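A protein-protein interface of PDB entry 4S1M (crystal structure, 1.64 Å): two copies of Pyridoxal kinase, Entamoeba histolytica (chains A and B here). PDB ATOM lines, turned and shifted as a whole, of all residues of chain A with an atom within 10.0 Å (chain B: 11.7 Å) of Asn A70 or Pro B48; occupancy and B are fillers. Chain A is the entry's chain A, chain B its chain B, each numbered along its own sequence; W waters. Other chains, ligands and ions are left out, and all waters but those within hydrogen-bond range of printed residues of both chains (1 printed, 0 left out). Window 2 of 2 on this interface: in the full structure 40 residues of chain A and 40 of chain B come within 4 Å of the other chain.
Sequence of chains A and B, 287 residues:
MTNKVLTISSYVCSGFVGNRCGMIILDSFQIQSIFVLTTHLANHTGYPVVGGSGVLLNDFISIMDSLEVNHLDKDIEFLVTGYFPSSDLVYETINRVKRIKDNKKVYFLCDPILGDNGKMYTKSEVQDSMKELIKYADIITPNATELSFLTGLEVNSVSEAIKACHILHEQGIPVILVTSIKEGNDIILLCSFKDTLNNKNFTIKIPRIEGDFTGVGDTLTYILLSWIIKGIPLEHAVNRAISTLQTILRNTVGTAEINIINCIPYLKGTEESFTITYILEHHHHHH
The side-chain amide nitrogen (ND2) of Asn A70 is in hydrogen-bond range of the backbone carbonyl oxygen (O) of Val B49 (2.9 Å).
OG of Ser A66 lies within hydrogen-bond range of N of Gly B51 (3.0 Å).
ND2 of Asn A70 is in hydrogen-bond range of OD1 of Asn B43 (3.0 Å).
The side-chain amide nitrogen (ND2) of Asn A3 lies within hydrogen-bond range of the side-chain hydroxyl (OG) of Ser B14 (3.0 Å).
OG of Ser A66 is in hydrogen-bond range of OD1 of Asn B43 (2.8 Å).
The side-chain hydroxyl of Ser A66 sits at hydrogen-bond distance from the backbone carbonyl oxygen of Val B49 (3.3 Å).
The side-chain hydroxyl (OG) of Ser A62 sits at hydrogen-bond distance from the backbone NH (N) of Gly B52, at 3.0 Å.
No position is printed for both chains.
Of the 20 pairs that touch across the chains among the printed residues, none has its exchanged pair printed and touching as well.
Among the printed residues, merely in contact across the chains: Ile A34 with Cys B13, Ser A62 with Gly B51, Ile A63 with Ala B42, Ile A63 with Gly B51, Ile A63 with Gly B52, Ser A66 with Ala B42, Ser A66 with Val B50, Leu A67 with Ser B14, Leu A67 with Ala B42, Asn A70 with Tyr B47, Asn A70 with Pro B48, Leu A72 with Asn B43 and Leu A72 with Tyr B47.
Asn A70 touches just these residues of chain B: Asn B43, Tyr B47, Pro B48 and Val B49.
Pro B48 touches just one residue of chain A: Asn A70.
Of chain B, only Ala B42 (3.5 Å), Asn B43 (2.8 Å), Val B49 (3.3 Å), Val B50 (3.8 Å) and Gly B51 (3.0 Å) come within 4 Å of Ser A66.
No residue of chain B comes within 4 Å of Val A69.
His A71 touches none of the printed residues of chain B.
Leu A72 touches two residues of chain B.
Val B49 touches just these residues of chain A: Ser A66 (3.3 Å) and Asn A70 (2.9 Å).
Printed residues of chain B within 4 Å of Ser A62: Gly B51 (3.2 Å) and Gly B52 (3.0 Å).
Of the printed residues of chain A, Asn B43 touches Ser A66, Asn A70 and Leu A72.
Printed residues of chain B within 4 Å of Ile A34: Cys B13.
Of the printed residues of chain A, Tyr B47 touches Asn A70 (3.6 Å) and Leu A72 (3.8 Å).
Ala B256 touches none of the printed residues of chain A.
Water W1 bridges the side-chain amide oxygen of Asn A3 (2.7 Å) and the backbone NH of Gly B15 (3.0 Å).
Of the 16 printed residues of chain A, 8 touch a printed residue of chain B.
Hydrophobic or aromatic side chains of chain A within 4 Å of the printed part of chain B: Ile A34, Ile A63, Leu A67 and Leu A72.
Of the 19 printed residues of chain B, 10 touch a printed residue of chain A.
Among the printed residues, 20 pairs touch across the chains.
Among the printed residues, no Asp or Glu carboxylate lies within 4 Å of a Lys or Arg side-chain nitrogen of the other chain.
N of Leu A72 is in hydrogen-bond range of O of Leu A67 (2.9 Å).
O of Ser A66 lies within hydrogen-bond range of ND2 of Asn A70 (3.1 Å).
The backbone NH of Cys B13 sits at hydrogen-bond distance from the backbone carbonyl oxygen of Leu B41 (2.8 Å).
The side-chain hydroxyl (OH) of Tyr B47 lies within hydrogen-bond range of the side-chain carboxylate (OE2) of Glu B257 (2.9 Å).
O of Val B49 sits at hydrogen-bond distance from ND2 of Asn B43, 3.0 Å away.
N of Cys B13 lies within hydrogen-bond range of O of Ala B42, at 3.4 Å.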
ATOM      1  N   ASN A   3      10.180  -5.220 -30.752  1.00  0.00           N
ATOM      2  CA  ASN A   3      10.253  -5.312 -29.321  1.00  0.00           C
ATOM      3  C   ASN A   3      11.535  -6.033 -28.895  1.00  0.00           C
ATOM      4  O   ASN A   3      11.803  -7.138 -29.314  1.00  0.00           O
ATOM      5  CB  ASN A   3       9.051  -6.045 -28.748  1.00  0.00           C
ATOM      6  CG  ASN A   3       7.756  -5.259 -28.948  1.00  0.00           C
ATOM      7  OD1 ASN A   3       7.701  -4.102 -28.613  1.00  0.00           O
ATOM      8  ND2 ASN A   3       6.718  -5.919 -29.423  1.00  0.00           N
ATOM      9  N   ILE A  34       7.663  -4.817 -24.285  1.00  0.00           N
ATOM     10  CA  ILE A  34       6.312  -5.323 -24.060  1.00  0.00           C
ATOM     11  C   ILE A  34       6.104  -5.354 -22.554  1.00  0.00           C
ATOM     12  O   ILE A  34       6.940  -5.945 -21.823  1.00  0.00           O
ATOM     13  CB  ILE A  34       6.177  -6.736 -24.597  1.00  0.00           C
ATOM     14  CG1 ILE A  34       6.468  -6.824 -26.076  1.00  0.00           C
ATOM     15  CG2 ILE A  34       4.769  -7.248 -24.281  1.00  0.00           C
ATOM     16  CD1 ILE A  34       6.625  -8.266 -26.565  1.00  0.00           C
ATOM     17  N   SER A  62      -3.749 -16.106 -22.445  1.00  0.00           N
ATOM     18  CA  SER A  62      -4.307 -15.512 -23.649  1.00  0.00           C
ATOM     19  C   SER A  62      -3.390 -14.419 -24.199  1.00  0.00           C
ATOM     20  O   SER A  62      -3.163 -14.344 -25.398  1.00  0.00           O
ATOM     21  CB  SER A  62      -5.676 -14.904 -23.361  1.00  0.00           C
ATOM     22  OG  SER A  62      -6.283 -14.396 -24.525  1.00  0.00           O
ATOM     23  N   ILE A  63      -2.887 -13.591 -23.286  1.00  0.00           N
ATOM     24  CA  ILE A  63      -1.954 -12.546 -23.689  1.00  0.00           C
ATOM     25  C   ILE A  63      -0.662 -13.083 -24.257  1.00  0.00           C
ATOM     26  O   ILE A  63      -0.222 -12.694 -25.339  1.00  0.00           O
ATOM     27  CB  ILE A  63      -1.665 -11.571 -22.501  1.00  0.00           C
ATOM     28  CG1 ILE A  63      -2.936 -10.743 -22.253  1.00  0.00           C
ATOM     29  CG2 ILE A  63      -0.478 -10.711 -22.794  1.00  0.00           C
ATOM     30  CD1 ILE A  63      -2.915  -9.977 -20.941  1.00  0.00           C
ATOM     31  N   MET A  64      -0.047 -14.000 -23.524  1.00  0.00           N
ATOM     32  CA  MET A  64       1.253 -14.520 -23.972  1.00  0.00           C
ATOM     33  C   MET A  64       1.060 -15.281 -25.321  1.00  0.00           C
ATOM     34  O   MET A  64       1.882 -15.132 -26.224  1.00  0.00           O
ATOM     35  CB  MET A  64       1.868 -15.467 -22.911  1.00  0.00           C
ATOM     36  CG  MET A  64       2.250 -14.778 -21.599  1.00  0.00           C
ATOM     37  SD  MET A  64       3.431 -13.447 -21.803  1.00  0.00           S
ATOM     38  CE  MET A  64       4.880 -14.434 -22.056  1.00  0.00           C
ATOM     39  N   ASP A  65      -0.032 -16.045 -25.463  1.00  0.00           N
ATOM     40  CA  ASP A  65      -0.305 -16.686 -26.723  1.00  0.00           C
ATOM     41  C   ASP A  65      -0.458 -15.673 -27.882  1.00  0.00           C
ATOM     42  O   ASP A  65       0.036 -15.894 -29.013  1.00  0.00           O
ATOM     43  CB  ASP A  65      -1.590 -17.518 -26.645  1.00  0.00           C
ATOM     44  CG  ASP A  65      -1.420 -18.828 -25.898  1.00  0.00           C
ATOM     45  OD1 ASP A  65      -0.285 -19.194 -25.531  1.00  0.00           O
ATOM     46  OD2 ASP A  65      -2.519 -19.422 -25.739  1.00  0.00           O
ATOM     47  N   SER A  66      -1.154 -14.572 -27.612  1.00  0.00           N
ATOM     48  CA  SER A  66      -1.393 -13.558 -28.642  1.00  0.00           C
ATOM     49  C   SER A  66      -0.062 -12.910 -29.118  1.00  0.00           C
ATOM     50  O   SER A  66       0.169 -12.699 -30.309  1.00  0.00           O
ATOM     51  CB  SER A  66      -2.346 -12.513 -28.088  1.00  0.00           C
ATOM     52  OG  SER A  66      -2.766 -11.543 -29.041  1.00  0.00           O
ATOM     53  N   LEU A  67       0.780 -12.572 -28.157  1.00  0.00           N
ATOM     54  CA  LEU A  67       2.103 -12.019 -28.480  1.00  0.00           C
ATOM     55  C   LEU A  67       2.881 -12.959 -29.349  1.00  0.00           C
ATOM     56  O   LEU A  67       3.472 -12.523 -30.311  1.00  0.00           O
ATOM     57  CB  LEU A  67       2.901 -11.711 -27.199  1.00  0.00           C
ATOM     58  CG  LEU A  67       2.299 -10.681 -26.265  1.00  0.00           C
ATOM     59  CD1 LEU A  67       3.056 -10.684 -24.936  1.00  0.00           C
ATOM     60  CD2 LEU A  67       2.276  -9.293 -26.936  1.00  0.00           C
ATOM     61  N   GLU A  68       2.863 -14.255 -29.010  1.00  0.00           N
ATOM     62  CA  GLU A  68       3.603 -15.223 -29.804  1.00  0.00           C
ATOM     63  C   GLU A  68       3.022 -15.408 -31.204  1.00  0.00           C
ATOM     64  O   GLU A  68       3.760 -15.363 -32.195  1.00  0.00           O
ATOM     65  CB  GLU A  68       3.660 -16.527 -29.047  1.00  0.00           C
ATOM     66  CG  GLU A  68       4.371 -17.658 -29.753  1.00  0.00           C
ATOM     67  CD  GLU A  68       4.570 -18.919 -28.922  1.00  0.00           C
ATOM     68  OE1 GLU A  68       4.306 -18.918 -27.695  1.00  0.00           O
ATOM     69  OE2 GLU A  68       5.051 -19.916 -29.567  1.00  0.00           O
ATOM     70  N   VAL A  69       1.715 -15.602 -31.308  1.00  0.00           N
ATOM     71  CA  VAL A  69       1.098 -15.899 -32.612  1.00  0.00           C
ATOM     72  C   VAL A  69       1.246 -14.714 -33.558  1.00  0.00           C
ATOM     73  O   VAL A  69       1.451 -14.898 -34.760  1.00  0.00           O
ATOM     74  CB  VAL A  69      -0.372 -16.334 -32.437  1.00  0.00           C
ATOM     75  CG1 VAL A  69      -1.035 -16.568 -33.782  1.00  0.00           C
ATOM     76  CG2 VAL A  69      -0.388 -17.630 -31.665  1.00  0.00           C
ATOM     77  N   ASN A  70       1.171 -13.496 -33.001  1.00  0.00           N
ATOM     78  CA  ASN A  70       1.326 -12.256 -33.811  1.00  0.00           C
ATOM     79  C   ASN A  70       2.792 -11.869 -34.036  1.00  0.00           C
ATOM     80  O   ASN A  70       3.075 -10.835 -34.631  1.00  0.00           O
ATOM     81  CB  ASN A  70       0.574 -11.111 -33.176  1.00  0.00           C
ATOM     82  CG  ASN A  70      -0.910 -11.298 -33.207  1.00  0.00           C
ATOM     83  OD1 ASN A  70      -1.482 -11.746 -34.202  1.00  0.00           O
ATOM     84  ND2 ASN A  70      -1.554 -10.884 -32.163  1.00  0.00           N
ATOM     85  N   HIS A  71       3.729 -12.708 -33.586  1.00  0.00           N
ATOM     86  CA  HIS A  71       5.173 -12.528 -33.766  1.00  0.00           C
ATOM     87  C   HIS A  71       5.713 -11.276 -33.055  1.00  0.00           C
ATOM     88  O   HIS A  71       6.750 -10.787 -33.412  1.00  0.00           O
ATOM     89  CB  HIS A  71       5.541 -12.572 -35.258  1.00  0.00           C
ATOM     90  CG  HIS A  71       5.174 -13.884 -35.909  1.00  0.00           C
ATOM     91  ND1 HIS A  71       5.849 -15.045 -35.623  1.00  0.00           N
ATOM     92  CD2 HIS A  71       4.188 -14.229 -36.774  1.00  0.00           C
ATOM     93  CE1 HIS A  71       5.335 -16.047 -36.310  1.00  0.00           C
ATOM     94  NE2 HIS A  71       4.311 -15.583 -37.006  1.00  0.00           N
ATOM     95  N   LEU A  72       5.022 -10.828 -32.013  1.00  0.00           N
ATOM     96  CA  LEU A  72       5.410  -9.586 -31.318  1.00  0.00           C
ATOM     97  C   LEU A  72       6.528  -9.778 -30.339  1.00  0.00           C
ATOM     98  O   LEU A  72       7.159  -8.798 -29.963  1.00  0.00           O
ATOM     99  CB  LEU A  72       4.191  -8.924 -30.681  1.00  0.00           C
ATOM    100  CG  LEU A  72       3.100  -8.511 -31.672  1.00  0.00           C
ATOM    101  CD1 LEU A  72       1.855  -8.105 -30.952  1.00  0.00           C
ATOM    102  CD2 LEU A  72       3.583  -7.376 -32.555  1.00  0.00           C
ATOM    103  N   ASP A  73       6.856 -11.044 -30.028  1.00  0.00           N
ATOM    104  CA  ASP A  73       7.939 -11.381 -29.133  1.00  0.00           C
ATOM    105  C   ASP A  73       9.035 -12.146 -29.835  1.00  0.00           C
ATOM    106  O   ASP A  73       9.979 -12.651 -29.161  1.00  0.00           O
ATOM    107  CB  ASP A  73       7.405 -12.200 -27.962  1.00  0.00           C
ATOM    108  CG  ASP A  73       6.848 -13.555 -28.417  1.00  0.00           C
ATOM    109  OD1 ASP A  73       6.890 -13.834 -29.621  1.00  0.00           O
ATOM    110  OD2 ASP A  73       6.453 -14.364 -27.566  1.00  0.00           O
ATOM    111  N   LYS A  74       9.032 -12.130 -31.161  1.00  0.00           N
ATOM    112  CA  LYS A  74       9.960 -12.942 -31.956  1.00  0.00           C
ATOM    113  C   LYS A  74      11.421 -12.501 -31.785  1.00  0.00           C
ATOM    114  O   LYS A  74      12.311 -13.342 -31.826  1.00  0.00           O
ATOM    115  CB  LYS A  74       9.572 -12.842 -33.429  1.00  0.00           C
ATOM    116  CG  LYS A  74      10.159 -13.879 -34.321  1.00  0.00           C
ATOM    117  CD  LYS A  74       9.441 -13.899 -35.687  1.00  0.00           C
ATOM    118  CE  LYS A  74      10.418 -14.240 -36.806  1.00  0.00           C
ATOM    119  NZ  LYS A  74      11.644 -13.380 -36.842  1.00  0.00           N
ATOM    120  N   ASP A  75      11.639 -11.200 -31.549  1.00  0.00           N
ATOM    121  CA  ASP A  75      12.952 -10.564 -31.535  1.00  0.00           C
ATOM    122  C   ASP A  75      13.432 -10.115 -30.167  1.00  0.00           C
ATOM    123  O   ASP A  75      14.421  -9.393 -30.055  1.00  0.00           O
ATOM    124  CB  ASP A  75      12.910  -9.365 -32.462  1.00  0.00           C
ATOM    125  CG  ASP A  75      12.485  -9.762 -33.891  1.00  0.00           C
ATOM    126  OD1 ASP A  75      13.060 -10.746 -34.402  1.00  0.00           O
ATOM    127  OD2 ASP A  75      11.542  -9.124 -34.442  1.00  0.00           O
ATOM    128  N   VAL B  12      -2.753  -1.835 -23.985  1.00  0.00           N
ATOM    129  CA  VAL B  12      -2.207  -2.916 -24.730  1.00  0.00           C
ATOM    130  C   VAL B  12      -0.739  -3.145 -24.219  1.00  0.00           C
ATOM    131  O   VAL B  12       0.000  -2.189 -23.930  1.00  0.00           O
ATOM    132  CB  VAL B  12      -2.148  -2.662 -26.232  1.00  0.00           C
ATOM    133  CG1 VAL B  12      -3.537  -2.759 -26.808  1.00  0.00           C
ATOM    134  CG2 VAL B  12      -1.475  -1.338 -26.547  1.00  0.00           C
ATOM    135  N   CYS B  13      -0.339  -4.417 -24.144  1.00  0.00           N
ATOM    136  CA  CYS B  13       0.980  -4.765 -23.626  1.00  0.00           C
ATOM    137  C   CYS B  13       2.077  -4.419 -24.609  1.00  0.00           C
ATOM    138  O   CYS B  13       3.207  -4.018 -24.203  1.00  0.00           O
ATOM    139  CB  CYS B  13       1.103  -6.226 -23.236  1.00  0.00           C
ATOM    140  SG  CYS B  13      -0.069  -6.771 -21.994  1.00  0.00           S
ATOM    141  N   SER B  14       1.824  -4.627 -25.890  1.00  0.00           N
ATOM    142  CA  SER B  14       2.712  -4.312 -26.981  1.00  0.00           C
ATOM    143  C   SER B  14       2.032  -3.228 -27.808  1.00  0.00           C
ATOM    144  O   SER B  14       0.808  -3.298 -27.997  1.00  0.00           O
ATOM    145  CB  SER B  14       2.860  -5.511 -27.875  1.00  0.00           C
ATOM    146  OG  SER B  14       3.819  -5.270 -28.882  1.00  0.00           O
ATOM    147  N   GLY B  15       2.806  -2.253 -28.293  1.00  0.00           N
ATOM    148  CA  GLY B  15       2.254  -1.182 -29.093  1.00  0.00           C
ATOM    149  C   GLY B  15       1.561  -0.076 -28.341  1.00  0.00           C
ATOM    150  O   GLY B  15       1.603  -0.019 -27.116  1.00  0.00           O
ATOM    151  N   LEU B  41      -5.051  -5.994 -22.857  1.00  0.00           N
ATOM    152  CA  LEU B  41      -4.917  -6.777 -24.029  1.00  0.00           C
ATOM    153  C   LEU B  41      -3.466  -6.926 -24.439  1.00  0.00           C
ATOM    154  O   LEU B  41      -2.647  -6.046 -24.140  1.00  0.00           O
ATOM    155  CB  LEU B  41      -5.657  -6.089 -25.193  1.00  0.00           C
ATOM    156  CG  LEU B  41      -7.102  -5.749 -24.926  1.00  0.00           C
ATOM    157  CD1 LEU B  41      -7.610  -4.954 -26.152  1.00  0.00           C
ATOM    158  CD2 LEU B  41      -7.900  -7.018 -24.675  1.00  0.00           C
ATOM    159  N   ALA B  42      -3.172  -7.990 -25.155  1.00  0.00           N
ATOM    160  CA  ALA B  42      -1.807  -8.230 -25.652  1.00  0.00           C
ATOM    161  C   ALA B  42      -1.320  -7.138 -26.629  1.00  0.00           C
ATOM    162  O   ALA B  42      -0.171  -6.745 -26.648  1.00  0.00           O
ATOM    163  CB  ALA B  42      -1.690  -9.586 -26.276  1.00  0.00           C
ATOM    164  N   ASN B  43      -2.252  -6.755 -27.490  1.00  0.00           N
ATOM    165  CA  ASN B  43      -1.965  -5.963 -28.652  1.00  0.00           C
ATOM    166  C   ASN B  43      -3.303  -5.372 -29.140  1.00  0.00           C
ATOM    167  O   ASN B  43      -4.371  -5.705 -28.640  1.00  0.00           O
ATOM    168  CB  ASN B  43      -1.278  -6.771 -29.684  1.00  0.00           C
ATOM    169  CG  ASN B  43      -1.958  -8.105 -29.961  1.00  0.00           C
ATOM    170  OD1 ASN B  43      -1.465  -9.181 -29.644  1.00  0.00           O
ATOM    171  ND2 ASN B  43      -3.123  -8.023 -30.621  1.00  0.00           N
ATOM    172  N   HIS B  44      -3.181  -4.424 -30.057  1.00  0.00           N
ATOM    173  CA  HIS B  44      -4.400  -3.769 -30.553  1.00  0.00           C
ATOM    174  C   HIS B  44      -5.208  -4.694 -31.447  1.00  0.00           C
ATOM    175  O   HIS B  44      -4.801  -5.753 -31.888  1.00  0.00           O
ATOM    176  CB  HIS B  44      -4.099  -2.401 -31.145  1.00  0.00           C
ATOM    177  CG  HIS B  44      -3.287  -2.435 -32.358  1.00  0.00           C
ATOM    178  ND1 HIS B  44      -3.674  -3.072 -33.510  1.00  0.00           N
ATOM    179  CD2 HIS B  44      -2.147  -1.781 -32.663  1.00  0.00           C
ATOM    180  CE1 HIS B  44      -2.741  -2.952 -34.428  1.00  0.00           C
ATOM    181  NE2 HIS B  44      -1.811  -2.145 -33.940  1.00  0.00           N
ATOM    182  N   THR B  45      -6.412  -4.200 -31.779  1.00  0.00           N
ATOM    183  CA  THR B  45      -7.383  -5.003 -32.474  1.00  0.00           C
ATOM    184  C   THR B  45      -7.140  -5.149 -33.983  1.00  0.00           C
ATOM    185  O   THR B  45      -7.852  -5.856 -34.681  1.00  0.00           O
ATOM    186  CB  THR B  45      -8.818  -4.492 -32.142  1.00  0.00           C
ATOM    187  OG1 THR B  45      -8.876  -3.115 -32.451  1.00  0.00           O
ATOM    188  CG2 THR B  45      -9.175  -4.669 -30.644  1.00  0.00           C
ATOM    189  N   GLY B  46      -6.135  -4.498 -34.529  1.00  0.00           N
ATOM    190  CA  GLY B  46      -5.624  -4.740 -35.844  1.00  0.00           C
ATOM    191  C   GLY B  46      -5.034  -6.079 -36.223  1.00  0.00           C
ATOM    192  O   GLY B  46      -5.006  -6.423 -37.388  1.00  0.00           O
ATOM    193  N   TYR B  47      -4.597  -6.864 -35.245  1.00  0.00           N
ATOM    194  CA  TYR B  47      -4.055  -8.155 -35.443  1.00  0.00           C
ATOM    195  C   TYR B  47      -5.171  -9.229 -35.506  1.00  0.00           C
ATOM    196  O   TYR B  47      -6.237  -9.020 -34.899  1.00  0.00           O
ATOM    197  CB  TYR B  47      -3.064  -8.455 -34.267  1.00  0.00           C
ATOM    198  CG  TYR B  47      -1.851  -7.513 -34.220  1.00  0.00           C
ATOM    199  CD1 TYR B  47      -0.664  -7.788 -34.926  1.00  0.00           C
ATOM    200  CD2 TYR B  47      -1.904  -6.334 -33.506  1.00  0.00           C
ATOM    201  CE1 TYR B  47       0.398  -6.855 -34.890  1.00  0.00           C
ATOM    202  CE2 TYR B  47      -0.858  -5.418 -33.468  1.00  0.00           C
ATOM    203  CZ  TYR B  47       0.314  -5.726 -34.185  1.00  0.00           C
ATOM    204  OH  TYR B  47       1.301  -4.753 -34.068  1.00  0.00           O
ATOM    205  N   PRO B  48      -4.899 -10.387 -36.112  1.00  0.00           N
ATOM    206  CA  PRO B  48      -5.841 -11.520 -36.164  1.00  0.00           C
ATOM    207  C   PRO B  48      -6.255 -12.041 -34.792  1.00  0.00           C
ATOM    208  O   PRO B  48      -7.278 -12.677 -34.663  1.00  0.00           O
ATOM    209  CB  PRO B  48      -5.048 -12.625 -36.862  1.00  0.00           C
ATOM    210  CG  PRO B  48      -3.950 -11.910 -37.564  1.00  0.00           C
ATOM    211  CD  PRO B  48      -3.627 -10.737 -36.789  1.00  0.00           C
ATOM    212  N   VAL B  49      -5.376 -11.877 -33.797  1.00  0.00           N
ATOM    213  CA  VAL B  49      -5.564 -12.473 -32.480  1.00  0.00           C
ATOM    214  C   VAL B  49      -5.371 -11.348 -31.518  1.00  0.00           C
ATOM    215  O   VAL B  49      -4.432 -10.543 -31.687  1.00  0.00           O
ATOM    216  CB  VAL B  49      -4.526 -13.617 -32.201  1.00  0.00           C
ATOM    217  CG1 VAL B  49      -4.606 -14.016 -30.742  1.00  0.00           C
ATOM    218  CG2 VAL B  49      -4.717 -14.838 -33.104  1.00  0.00           C
ATOM    219  N   VAL B  50      -6.294 -11.188 -30.568  1.00  0.00           N
ATOM    220  CA  VAL B  50      -6.253 -10.144 -29.586  1.00  0.00           C
ATOM    221  C   VAL B  50      -6.457 -10.742 -28.194  1.00  0.00           C
ATOM    222  O   VAL B  50      -7.569 -10.761 -27.657  1.00  0.00           O
ATOM    223  CB  VAL B  50      -7.281  -8.998 -29.829  1.00  0.00           C
ATOM    224  CG1 VAL B  50      -7.101  -7.828 -28.912  1.00  0.00           C
ATOM    225  CG2 VAL B  50      -7.234  -8.515 -31.268  1.00  0.00           C
ATOM    226  N   GLY B  51      -5.354 -11.209 -27.575  1.00  0.00           N
ATOM    227  CA  GLY B  51      -5.468 -11.893 -26.283  1.00  0.00           C
ATOM    228  C   GLY B  51      -5.731 -10.913 -25.168  1.00  0.00           C
ATOM    229  O   GLY B  51      -5.378  -9.735 -25.235  1.00  0.00           O
ATOM    230  N   GLY B  52      -6.341 -11.407 -24.108  1.00  0.00           N
ATOM    231  CA  GLY B  52      -6.647 -10.639 -22.937  1.00  0.00           C
ATOM    232  C   GLY B  52      -8.093 -10.215 -22.877  1.00  0.00           C
ATOM    233  O   GLY B  52      -8.888 -10.453 -23.823  1.00  0.00           O
ATOM    234  N   THR B 214      -3.635   2.910 -35.992  1.00  0.00           N
ATOM    235  CA  THR B 214      -4.522   2.462 -34.891  1.00  0.00           C
ATOM    236  C   THR B 214      -4.732   3.488 -33.683  1.00  0.00           C
ATOM    237  O   THR B 214      -5.895   3.798 -33.276  1.00  0.00           O
ATOM    238  CB  THR B 214      -4.021   1.057 -34.468  1.00  0.00           C
ATOM    239  OG1 THR B 214      -4.920   0.461 -33.520  1.00  0.00           O
ATOM    240  CG2 THR B 214      -2.612   1.163 -33.891  1.00  0.00           C
ATOM    241  N   ALA B 256       1.500  -0.844 -38.711  1.00  0.00           N
ATOM    242  CA  ALA B 256       1.086  -1.655 -37.575  1.00  0.00           C
ATOM    243  C   ALA B 256       1.036  -0.796 -36.294  1.00  0.00           C
ATOM    244  O   ALA B 256       0.037  -0.854 -35.559  1.00  0.00           O
ATOM    245  CB  ALA B 256       1.985  -2.882 -37.377  1.00  0.00           C
ATOM    246  N   GLU B 257       2.071   0.029 -36.076  1.00  0.00           N
ATOM    247  CA  GLU B 257       2.179   0.845 -34.844  1.00  0.00           C
ATOM    248  C   GLU B 257       2.803   2.194 -35.143  1.00  0.00           C
ATOM    249  O   GLU B 257       3.724   2.292 -35.976  1.00  0.00           O
ATOM    250  CB  GLU B 257       3.114   0.172 -33.822  1.00  0.00           C
ATOM    251  CG  GLU B 257       2.666  -1.223 -33.392  1.00  0.00           C
ATOM    252  CD  GLU B 257       1.435  -1.246 -32.476  1.00  0.00           C
ATOM    253  OE1 GLU B 257       0.991  -0.143 -31.927  1.00  0.00           O
ATOM    254  OE2 GLU B 257       1.025  -2.455 -32.244  1.00  0.00           O
HETATM  255  O   HOH W   1       5.739  -2.338 -27.857  1.00  0.00           O
